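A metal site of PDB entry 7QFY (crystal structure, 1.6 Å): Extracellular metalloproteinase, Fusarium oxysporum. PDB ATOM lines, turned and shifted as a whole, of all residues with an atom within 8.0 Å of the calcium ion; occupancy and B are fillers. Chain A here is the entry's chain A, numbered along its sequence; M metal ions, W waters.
The backbone NH of Val 130 sits close to the side-chain amide nitrogen of Asn 124, 3.4 Å away. The side-chain amide nitrogen of Asn 119 is in hydrogen-bond range of the backbone carbonyl oxygen of Phe 113, at 3.1 Å. The guanidinium group (NH1) of Arg 193 sits close to the side-chain carboxylate (OD1) of Asp 155, at 3.3 Å. OD2 of Asp 133 lies close to NH1 of Arg 193 (2.9 Å). OD2 of Asp 133 sits close to N of Gly 156 (2.9 Å). The backbone carbonyl oxygen (O) of Gln 121 is in hydrogen-bond range of the backbone NH (N) of Asp 133 (3.1 Å). NH1 of Arg 193 lies within hydrogen-bond range of O of Gly 118, 3.0 Å away. The guanidinium group of Arg 193 sits at hydrogen-bond distance from the backbone carbonyl oxygen of Gln 157 (2.9 Å).
NH1 of Arg 193 touches the calcium ion, 3.9 Å away. Five residues have an atom within 4 Å of the calcium ion: Asn 119, Val 130, Asp 133, Asp 155 and Arg 193. The nearest printed residue that does not touch the calcium ion is Asn 124 (4.2 Å).
O of Val 130 binds the calcium ion (2.3 Å). The backbone carbonyl oxygen (O) of Asn 119 is bound to the calcium ion (2.3 Å). Water W1 binds the calcium ion (2.3 Å). The calcium ion is bound by the side-chain carboxylate (OD1) of Asp 155 (2.4 Å). Water W2 is bound to the calcium ion (2.5 Å). The calcium ion is bound by OD1 of Asp 133, 2.5 Å away. The side-chain carboxylate (OD2) of Asp 133 is bound to the calcium ion (2.5 Å).
Water W1 lies within hydrogen-bond range of the side-chain amide oxygen (OD1) of Asn 124 (2.7 Å), the side-chain amide oxygen (OD1) of Asn 119 (2.8 Å) and the backbone NH (N) of Gln 121 (3.4 Å). Water W2 lies within hydrogen-bond range of the backbone carbonyl oxygen of Glu 115 (2.8 Å), the side-chain carboxylate of Asp 155 (2.9 Å), the backbone NH of Val 130 (3.2 Å) and the side-chain amide nitrogen of Asn 124 (3.3 Å).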
ATOM      1  N   PHE A 113     -10.634 -31.116 -25.019  1.00  0.00           N
ATOM      2  CA  PHE A 113      -9.170 -31.090 -25.219  1.00  0.00           C
ATOM      3  C   PHE A 113      -8.900 -31.099 -26.724  1.00  0.00           C
ATOM      4  O   PHE A 113      -8.551 -32.119 -27.327  1.00  0.00           O
ATOM      5  CB  PHE A 113      -8.500 -32.275 -24.538  1.00  0.00           C
ATOM      6  CG  PHE A 113      -6.981 -32.153 -24.428  1.00  0.00           C
ATOM      7  CD1 PHE A 113      -6.379 -30.936 -24.055  1.00  0.00           C
ATOM      8  CD2 PHE A 113      -6.169 -33.245 -24.642  1.00  0.00           C
ATOM      9  CE1 PHE A 113      -4.990 -30.832 -23.907  1.00  0.00           C
ATOM     10  CE2 PHE A 113      -4.780 -33.167 -24.484  1.00  0.00           C
ATOM     11  CZ  PHE A 113      -4.195 -31.968 -24.117  1.00  0.00           C
ATOM     12  N   THR A 114      -9.133 -29.944 -27.317  1.00  0.00           N
ATOM     13  CA  THR A 114      -9.036 -29.734 -28.757  1.00  0.00           C
ATOM     14  C   THR A 114      -7.710 -29.085 -29.144  1.00  0.00           C
ATOM     15  O   THR A 114      -6.830 -28.857 -28.297  1.00  0.00           O
ATOM     16  CB  THR A 114     -10.187 -28.849 -29.197  1.00  0.00           C
ATOM     17  OG1 THR A 114     -10.032 -27.607 -28.504  1.00  0.00           O
ATOM     18  CG2 THR A 114     -11.537 -29.498 -28.848  1.00  0.00           C
ATOM     19  N   GLU A 115      -7.584 -28.730 -30.423  1.00  0.00           N
ATOM     20  CA  GLU A 115      -6.391 -28.023 -30.892  1.00  0.00           C
ATOM     21  C   GLU A 115      -6.141 -26.734 -30.099  1.00  0.00           C
ATOM     22  O   GLU A 115      -5.011 -26.494 -29.624  1.00  0.00           O
ATOM     23  CB  GLU A 115      -6.568 -27.721 -32.377  1.00  0.00           C
ATOM     24  CG  GLU A 115      -6.620 -28.962 -33.270  1.00  0.00           C
ATOM     25  CD  GLU A 115      -8.017 -29.589 -33.459  1.00  0.00           C
ATOM     26  OE1 GLU A 115      -9.035 -29.145 -32.855  1.00  0.00           O
ATOM     27  OE2 GLU A 115      -8.093 -30.584 -34.223  1.00  0.00           O
ATOM     28  N   GLN A 116      -7.147 -25.884 -29.959  1.00  0.00           N
ATOM     29  CA  GLN A 116      -6.947 -24.614 -29.251  1.00  0.00           C
ATOM     30  C   GLN A 116      -6.733 -24.811 -27.751  1.00  0.00           C
ATOM     31  O   GLN A 116      -6.367 -23.849 -27.063  1.00  0.00           O
ATOM     32  CB  GLN A 116      -8.121 -23.661 -29.513  1.00  0.00           C
ATOM     33  CG  GLN A 116      -9.401 -24.014 -28.807  1.00  0.00           C
ATOM     34  CD  GLN A 116     -10.559 -23.058 -29.058  1.00  0.00           C
ATOM     35  OE1 GLN A 116     -10.386 -21.941 -29.509  1.00  0.00           O
ATOM     36  NE2 GLN A 116     -11.769 -23.512 -28.741  1.00  0.00           N
ATOM     37  N   ALA A 117      -6.954 -26.009 -27.231  1.00  0.00           N
ATOM     38  CA  ALA A 117      -6.720 -26.307 -25.816  1.00  0.00           C
ATOM     39  C   ALA A 117      -5.340 -26.910 -25.578  1.00  0.00           C
ATOM     40  O   ALA A 117      -5.007 -27.236 -24.418  1.00  0.00           O
ATOM     41  CB  ALA A 117      -7.804 -27.280 -25.295  1.00  0.00           C
ATOM     42  N   GLY A 118      -4.529 -27.048 -26.624  1.00  0.00           N
ATOM     43  CA  GLY A 118      -3.176 -27.545 -26.463  1.00  0.00           C
ATOM     44  C   GLY A 118      -3.037 -29.050 -26.546  1.00  0.00           C
ATOM     45  O   GLY A 118      -2.176 -29.611 -25.863  1.00  0.00           O
ATOM     46  N   ASN A 119      -3.852 -29.716 -27.374  1.00  0.00           N
ATOM     47  CA  ASN A 119      -3.812 -31.176 -27.454  1.00  0.00           C
ATOM     48  C   ASN A 119      -2.653 -31.656 -28.336  1.00  0.00           C
ATOM     49  O   ASN A 119      -1.778 -30.882 -28.736  1.00  0.00           O
ATOM     50  CB  ASN A 119      -5.175 -31.725 -27.897  1.00  0.00           C
ATOM     51  CG  ASN A 119      -5.462 -31.600 -29.388  1.00  0.00           C
ATOM     52  OD1 ASN A 119      -4.707 -31.023 -30.163  1.00  0.00           O
ATOM     53  ND2 ASN A 119      -6.596 -32.179 -29.796  1.00  0.00           N
ATOM     54  N   PHE A 120      -2.603 -32.975 -28.582  1.00  0.00           N
ATOM     55  CA  PHE A 120      -1.445 -33.635 -29.204  1.00  0.00           C
ATOM     56  C   PHE A 120      -1.839 -34.114 -30.607  1.00  0.00           C
ATOM     57  O   PHE A 120      -2.513 -35.140 -30.755  1.00  0.00           O
ATOM     58  CB  PHE A 120      -0.976 -34.815 -28.344  1.00  0.00           C
ATOM     59  CG  PHE A 120      -0.508 -34.434 -26.960  1.00  0.00           C
ATOM     60  CD1 PHE A 120       0.781 -34.005 -26.713  1.00  0.00           C
ATOM     61  CD2 PHE A 120      -1.390 -34.539 -25.876  1.00  0.00           C
ATOM     62  CE1 PHE A 120       1.188 -33.668 -25.423  1.00  0.00           C
ATOM     63  CE2 PHE A 120      -0.987 -34.206 -24.616  1.00  0.00           C
ATOM     64  CZ  PHE A 120       0.285 -33.782 -24.379  1.00  0.00           C
ATOM     65  N   GLN A 121      -1.411 -33.387 -31.634  1.00  0.00           N
ATOM     66  CA  GLN A 121      -1.733 -33.735 -33.013  1.00  0.00           C
ATOM     67  C   GLN A 121      -0.645 -33.206 -33.926  1.00  0.00           C
ATOM     68  O   GLN A 121      -0.088 -32.132 -33.709  1.00  0.00           O
ATOM     69  CB  GLN A 121      -3.066 -33.126 -33.476  1.00  0.00           C
ATOM     70  CG  GLN A 121      -4.270 -33.715 -32.755  1.00  0.00           C
ATOM     71  CD  GLN A 121      -5.589 -33.102 -33.109  1.00  0.00           C
ATOM     72  OE1 GLN A 121      -6.588 -33.418 -32.456  1.00  0.00           O
ATOM     73  NE2 GLN A 121      -5.624 -32.186 -34.081  1.00  0.00           N
ATOM     74  N   THR A 122      -0.384 -33.949 -34.992  1.00  0.00           N
ATOM     75  CA  THR A 122       0.507 -33.425 -36.032  1.00  0.00           C
ATOM     76  C   THR A 122      -0.099 -32.222 -36.745  1.00  0.00           C
ATOM     77  O   THR A 122       0.556 -31.187 -36.891  1.00  0.00           O
ATOM     78  CB  THR A 122       0.837 -34.532 -37.021  1.00  0.00           C
ATOM     79  OG1 THR A 122       1.648 -35.516 -36.393  1.00  0.00           O
ATOM     80  CG2 THR A 122       1.579 -33.966 -38.224  1.00  0.00           C
ATOM     81  N   ASN A 123      -1.348 -32.328 -37.202  1.00  0.00           N
ATOM     82  CA  ASN A 123      -1.986 -31.295 -38.005  1.00  0.00           C
ATOM     83  C   ASN A 123      -3.220 -30.793 -37.261  1.00  0.00           C
ATOM     84  O   ASN A 123      -4.108 -31.580 -36.912  1.00  0.00           O
ATOM     85  CB  ASN A 123      -2.334 -31.877 -39.381  1.00  0.00           C
ATOM     86  CG  ASN A 123      -3.019 -30.869 -40.310  1.00  0.00           C
ATOM     87  OD1 ASN A 123      -3.112 -29.672 -40.043  1.00  0.00           O
ATOM     88  ND2 ASN A 123      -3.491 -31.383 -41.445  1.00  0.00           N
ATOM     89  N   ASN A 124      -3.265 -29.490 -36.997  1.00  0.00           N
ATOM     90  CA  ASN A 124      -4.399 -28.883 -36.318  1.00  0.00           C
ATOM     91  C   ASN A 124      -5.410 -28.290 -37.272  1.00  0.00           C
ATOM     92  O   ASN A 124      -6.451 -27.779 -36.829  1.00  0.00           O
ATOM     93  CB  ASN A 124      -3.916 -27.818 -35.325  1.00  0.00           C
ATOM     94  CG  ASN A 124      -3.293 -28.408 -34.073  1.00  0.00           C
ATOM     95  OD1 ASN A 124      -3.086 -29.607 -33.970  1.00  0.00           O
ATOM     96  ND2 ASN A 124      -3.001 -27.561 -33.112  1.00  0.00           N
ATOM     97  N   GLY A 128      -6.477 -23.890 -34.522  1.00  0.00           N
ATOM     98  CA  GLY A 128      -5.794 -23.198 -33.444  1.00  0.00           C
ATOM     99  C   GLY A 128      -4.702 -24.049 -32.813  1.00  0.00           C
ATOM    100  O   GLY A 128      -4.427 -25.183 -33.217  1.00  0.00           O
ATOM    101  N   GLY A 129      -4.096 -23.466 -31.760  1.00  0.00           N
ATOM    102  CA  GLY A 129      -2.957 -24.087 -31.124  1.00  0.00           C
ATOM    103  C   GLY A 129      -1.773 -24.306 -32.056  1.00  0.00           C
ATOM    104  O   GLY A 129      -1.581 -23.625 -33.076  1.00  0.00           O
ATOM    105  N   VAL A 130      -0.944 -25.269 -31.671  1.00  0.00           N
ATOM    106  CA  VAL A 130       0.272 -25.612 -32.395  1.00  0.00           C
ATOM    107  C   VAL A 130       0.275 -27.122 -32.623  1.00  0.00           C
ATOM    108  O   VAL A 130      -0.019 -27.891 -31.692  1.00  0.00           O
ATOM    109  CB  VAL A 130       1.542 -25.183 -31.628  1.00  0.00           C
ATOM    110  CG1 VAL A 130       2.793 -25.405 -32.492  1.00  0.00           C
ATOM    111  CG2 VAL A 130       1.432 -23.713 -31.162  1.00  0.00           C
ATOM    112  N   GLY A 131       0.556 -27.533 -33.852  1.00  0.00           N
ATOM    113  CA  GLY A 131       0.642 -28.941 -34.194  1.00  0.00           C
ATOM    114  C   GLY A 131       2.041 -29.493 -34.043  1.00  0.00           C
ATOM    115  O   GLY A 131       2.826 -29.060 -33.188  1.00  0.00           O
ATOM    116  N   ASN A 132       2.367 -30.477 -34.888  1.00  0.00           N
ATOM    117  CA  ASN A 132       3.631 -31.185 -34.844  1.00  0.00           C
ATOM    118  C   ASN A 132       3.880 -31.848 -33.493  1.00  0.00           C
ATOM    119  O   ASN A 132       5.025 -32.019 -33.084  1.00  0.00           O
ATOM    120  CB  ASN A 132       4.816 -30.261 -35.179  1.00  0.00           C
ATOM    121  CG  ASN A 132       4.551 -29.364 -36.353  1.00  0.00           C
ATOM    122  OD1 ASN A 132       4.484 -28.146 -36.211  1.00  0.00           O
ATOM    123  ND2 ASN A 132       4.376 -29.950 -37.507  1.00  0.00           N
ATOM    124  N   ASP A 133       2.821 -32.265 -32.802  1.00  0.00           N
ATOM    125  CA  ASP A 133       3.003 -32.828 -31.465  1.00  0.00           C
ATOM    126  C   ASP A 133       2.032 -33.967 -31.184  1.00  0.00           C
ATOM    127  O   ASP A 133       1.482 -34.083 -30.080  1.00  0.00           O
ATOM    128  CB  ASP A 133       2.952 -31.718 -30.398  1.00  0.00           C
ATOM    129  CG  ASP A 133       1.588 -31.020 -30.246  1.00  0.00           C
ATOM    130  OD1 ASP A 133       0.630 -31.201 -31.029  1.00  0.00           O
ATOM    131  OD2 ASP A 133       1.529 -30.172 -29.308  1.00  0.00           O
ATOM    132  N   MET A 134       1.850 -34.857 -32.166  1.00  0.00           N
ATOM    133  CA  MET A 134       1.281 -36.174 -31.889  1.00  0.00           C
ATOM    134  C   MET A 134       2.034 -36.850 -30.748  1.00  0.00           C
ATOM    135  O   MET A 134       3.177 -36.496 -30.452  1.00  0.00           O
ATOM    136  CB  MET A 134       1.316 -37.063 -33.151  1.00  0.00           C
ATOM    137  CG  MET A 134       2.642 -37.738 -33.459  1.00  0.00           C
ATOM    138  SD  MET A 134       3.925 -36.588 -33.981  1.00  0.00           S
ATOM    139  CE  MET A 134       5.348 -37.258 -33.143  1.00  0.00           C
ATOM    140  N   ALA A 154       6.012 -28.367 -23.924  1.00  0.00           N
ATOM    141  CA  ALA A 154       5.023 -27.354 -24.271  1.00  0.00           C
ATOM    142  C   ALA A 154       4.415 -27.656 -25.641  1.00  0.00           C
ATOM    143  O   ALA A 154       4.961 -28.436 -26.435  1.00  0.00           O
ATOM    144  CB  ALA A 154       5.644 -25.952 -24.285  1.00  0.00           C
ATOM    145  N   ASP A 155       3.248 -27.034 -25.876  1.00  0.00           N
ATOM    146  CA  ASP A 155       2.526 -27.201 -27.123  1.00  0.00           C
ATOM    147  C   ASP A 155       3.467 -27.020 -28.311  1.00  0.00           C
ATOM    148  O   ASP A 155       4.242 -26.063 -28.366  1.00  0.00           O
ATOM    149  CB  ASP A 155       1.389 -26.161 -27.177  1.00  0.00           C
ATOM    150  CG  ASP A 155       0.236 -26.571 -28.075  1.00  0.00           C
ATOM    151  OD1 ASP A 155       0.149 -27.758 -28.389  1.00  0.00           O
ATOM    152  OD2 ASP A 155      -0.580 -25.693 -28.466  1.00  0.00           O
ATOM    153  N   GLY A 156       3.384 -27.943 -29.262  1.00  0.00           N
ATOM    154  CA  GLY A 156       4.195 -27.890 -30.462  1.00  0.00           C
ATOM    155  C   GLY A 156       5.343 -28.876 -30.484  1.00  0.00           C
ATOM    156  O   GLY A 156       6.027 -28.987 -31.515  1.00  0.00           O
ATOM    157  N   GLN A 157       5.573 -29.583 -29.370  1.00  0.00           N
ATOM    158  CA  GLN A 157       6.588 -30.619 -29.261  1.00  0.00           C
ATOM    159  C   GLN A 157       5.857 -31.861 -28.783  1.00  0.00           C
ATOM    160  O   GLN A 157       5.024 -31.767 -27.873  1.00  0.00           O
ATOM    161  CB  GLN A 157       7.689 -30.209 -28.263  1.00  0.00           C
ATOM    162  CG  GLN A 157       8.486 -28.951 -28.661  1.00  0.00           C
ATOM    163  CD  GLN A 157       9.282 -28.398 -27.494  1.00  0.00           C
ATOM    164  OE1 GLN A 157       9.140 -27.223 -27.125  1.00  0.00           O
ATOM    165  NE2 GLN A 157      10.108 -29.239 -26.889  1.00  0.00           N
ATOM    166  N   PRO A 158       6.126 -33.041 -29.367  1.00  0.00           N
ATOM    167  CA  PRO A 158       5.340 -34.232 -29.012  1.00  0.00           C
ATOM    168  C   PRO A 158       5.474 -34.661 -27.559  1.00  0.00           C
ATOM    169  O   PRO A 158       6.549 -34.616 -26.960  1.00  0.00           O
ATOM    170  CB  PRO A 158       5.891 -35.319 -29.956  1.00  0.00           C
ATOM    171  CG  PRO A 158       7.092 -34.770 -30.563  1.00  0.00           C
ATOM    172  CD  PRO A 158       7.105 -33.299 -30.437  1.00  0.00           C
ATOM    173  N   ARG A 193      -0.650 -29.987 -20.065  1.00  0.00           N
ATOM    174  CA  ARG A 193      -0.980 -29.007 -21.097  1.00  0.00           C
ATOM    175  C   ARG A 193      -2.008 -28.002 -20.589  1.00  0.00           C
ATOM    176  O   ARG A 193      -1.828 -26.797 -20.709  1.00  0.00           O
ATOM    177  CB  ARG A 193      -1.465 -29.688 -22.373  1.00  0.00           C
ATOM    178  CG  ARG A 193      -0.349 -30.375 -23.181  1.00  0.00           C
ATOM    179  CD  ARG A 193       0.546 -29.351 -23.881  1.00  0.00           C
ATOM    180  NE  ARG A 193       1.695 -29.954 -24.549  1.00  0.00           N
ATOM    181  CZ  ARG A 193       1.690 -30.392 -25.797  1.00  0.00           C
ATOM    182  NH1 ARG A 193       0.584 -30.419 -26.526  1.00  0.00           N
ATOM    183  NH2 ARG A 193       2.827 -30.801 -26.335  1.00  0.00           N
ATOM    184  N   PRO A 198      -1.239 -24.073 -22.578  1.00  0.00           N
ATOM    185  CA  PRO A 198      -0.433 -25.082 -23.287  1.00  0.00           C
ATOM    186  C   PRO A 198       1.041 -24.750 -23.418  1.00  0.00           C
ATOM    187  O   PRO A 198       1.825 -25.657 -23.740  1.00  0.00           O
ATOM    188  CB  PRO A 198      -1.092 -25.149 -24.672  1.00  0.00           C
ATOM    189  CG  PRO A 198      -2.490 -24.661 -24.459  1.00  0.00           C
ATOM    190  CD  PRO A 198      -2.326 -23.567 -23.418  1.00  0.00           C
HETATM  191 CA    CA M   1      -0.704 -29.315 -30.064  1.00  0.00          CA
HETATM  192  O   HOH W   1      -2.368 -30.152 -31.450  1.00  0.00           O
HETATM  193  O   HOH W   2      -2.367 -27.516 -29.853  1.00  0.00           O
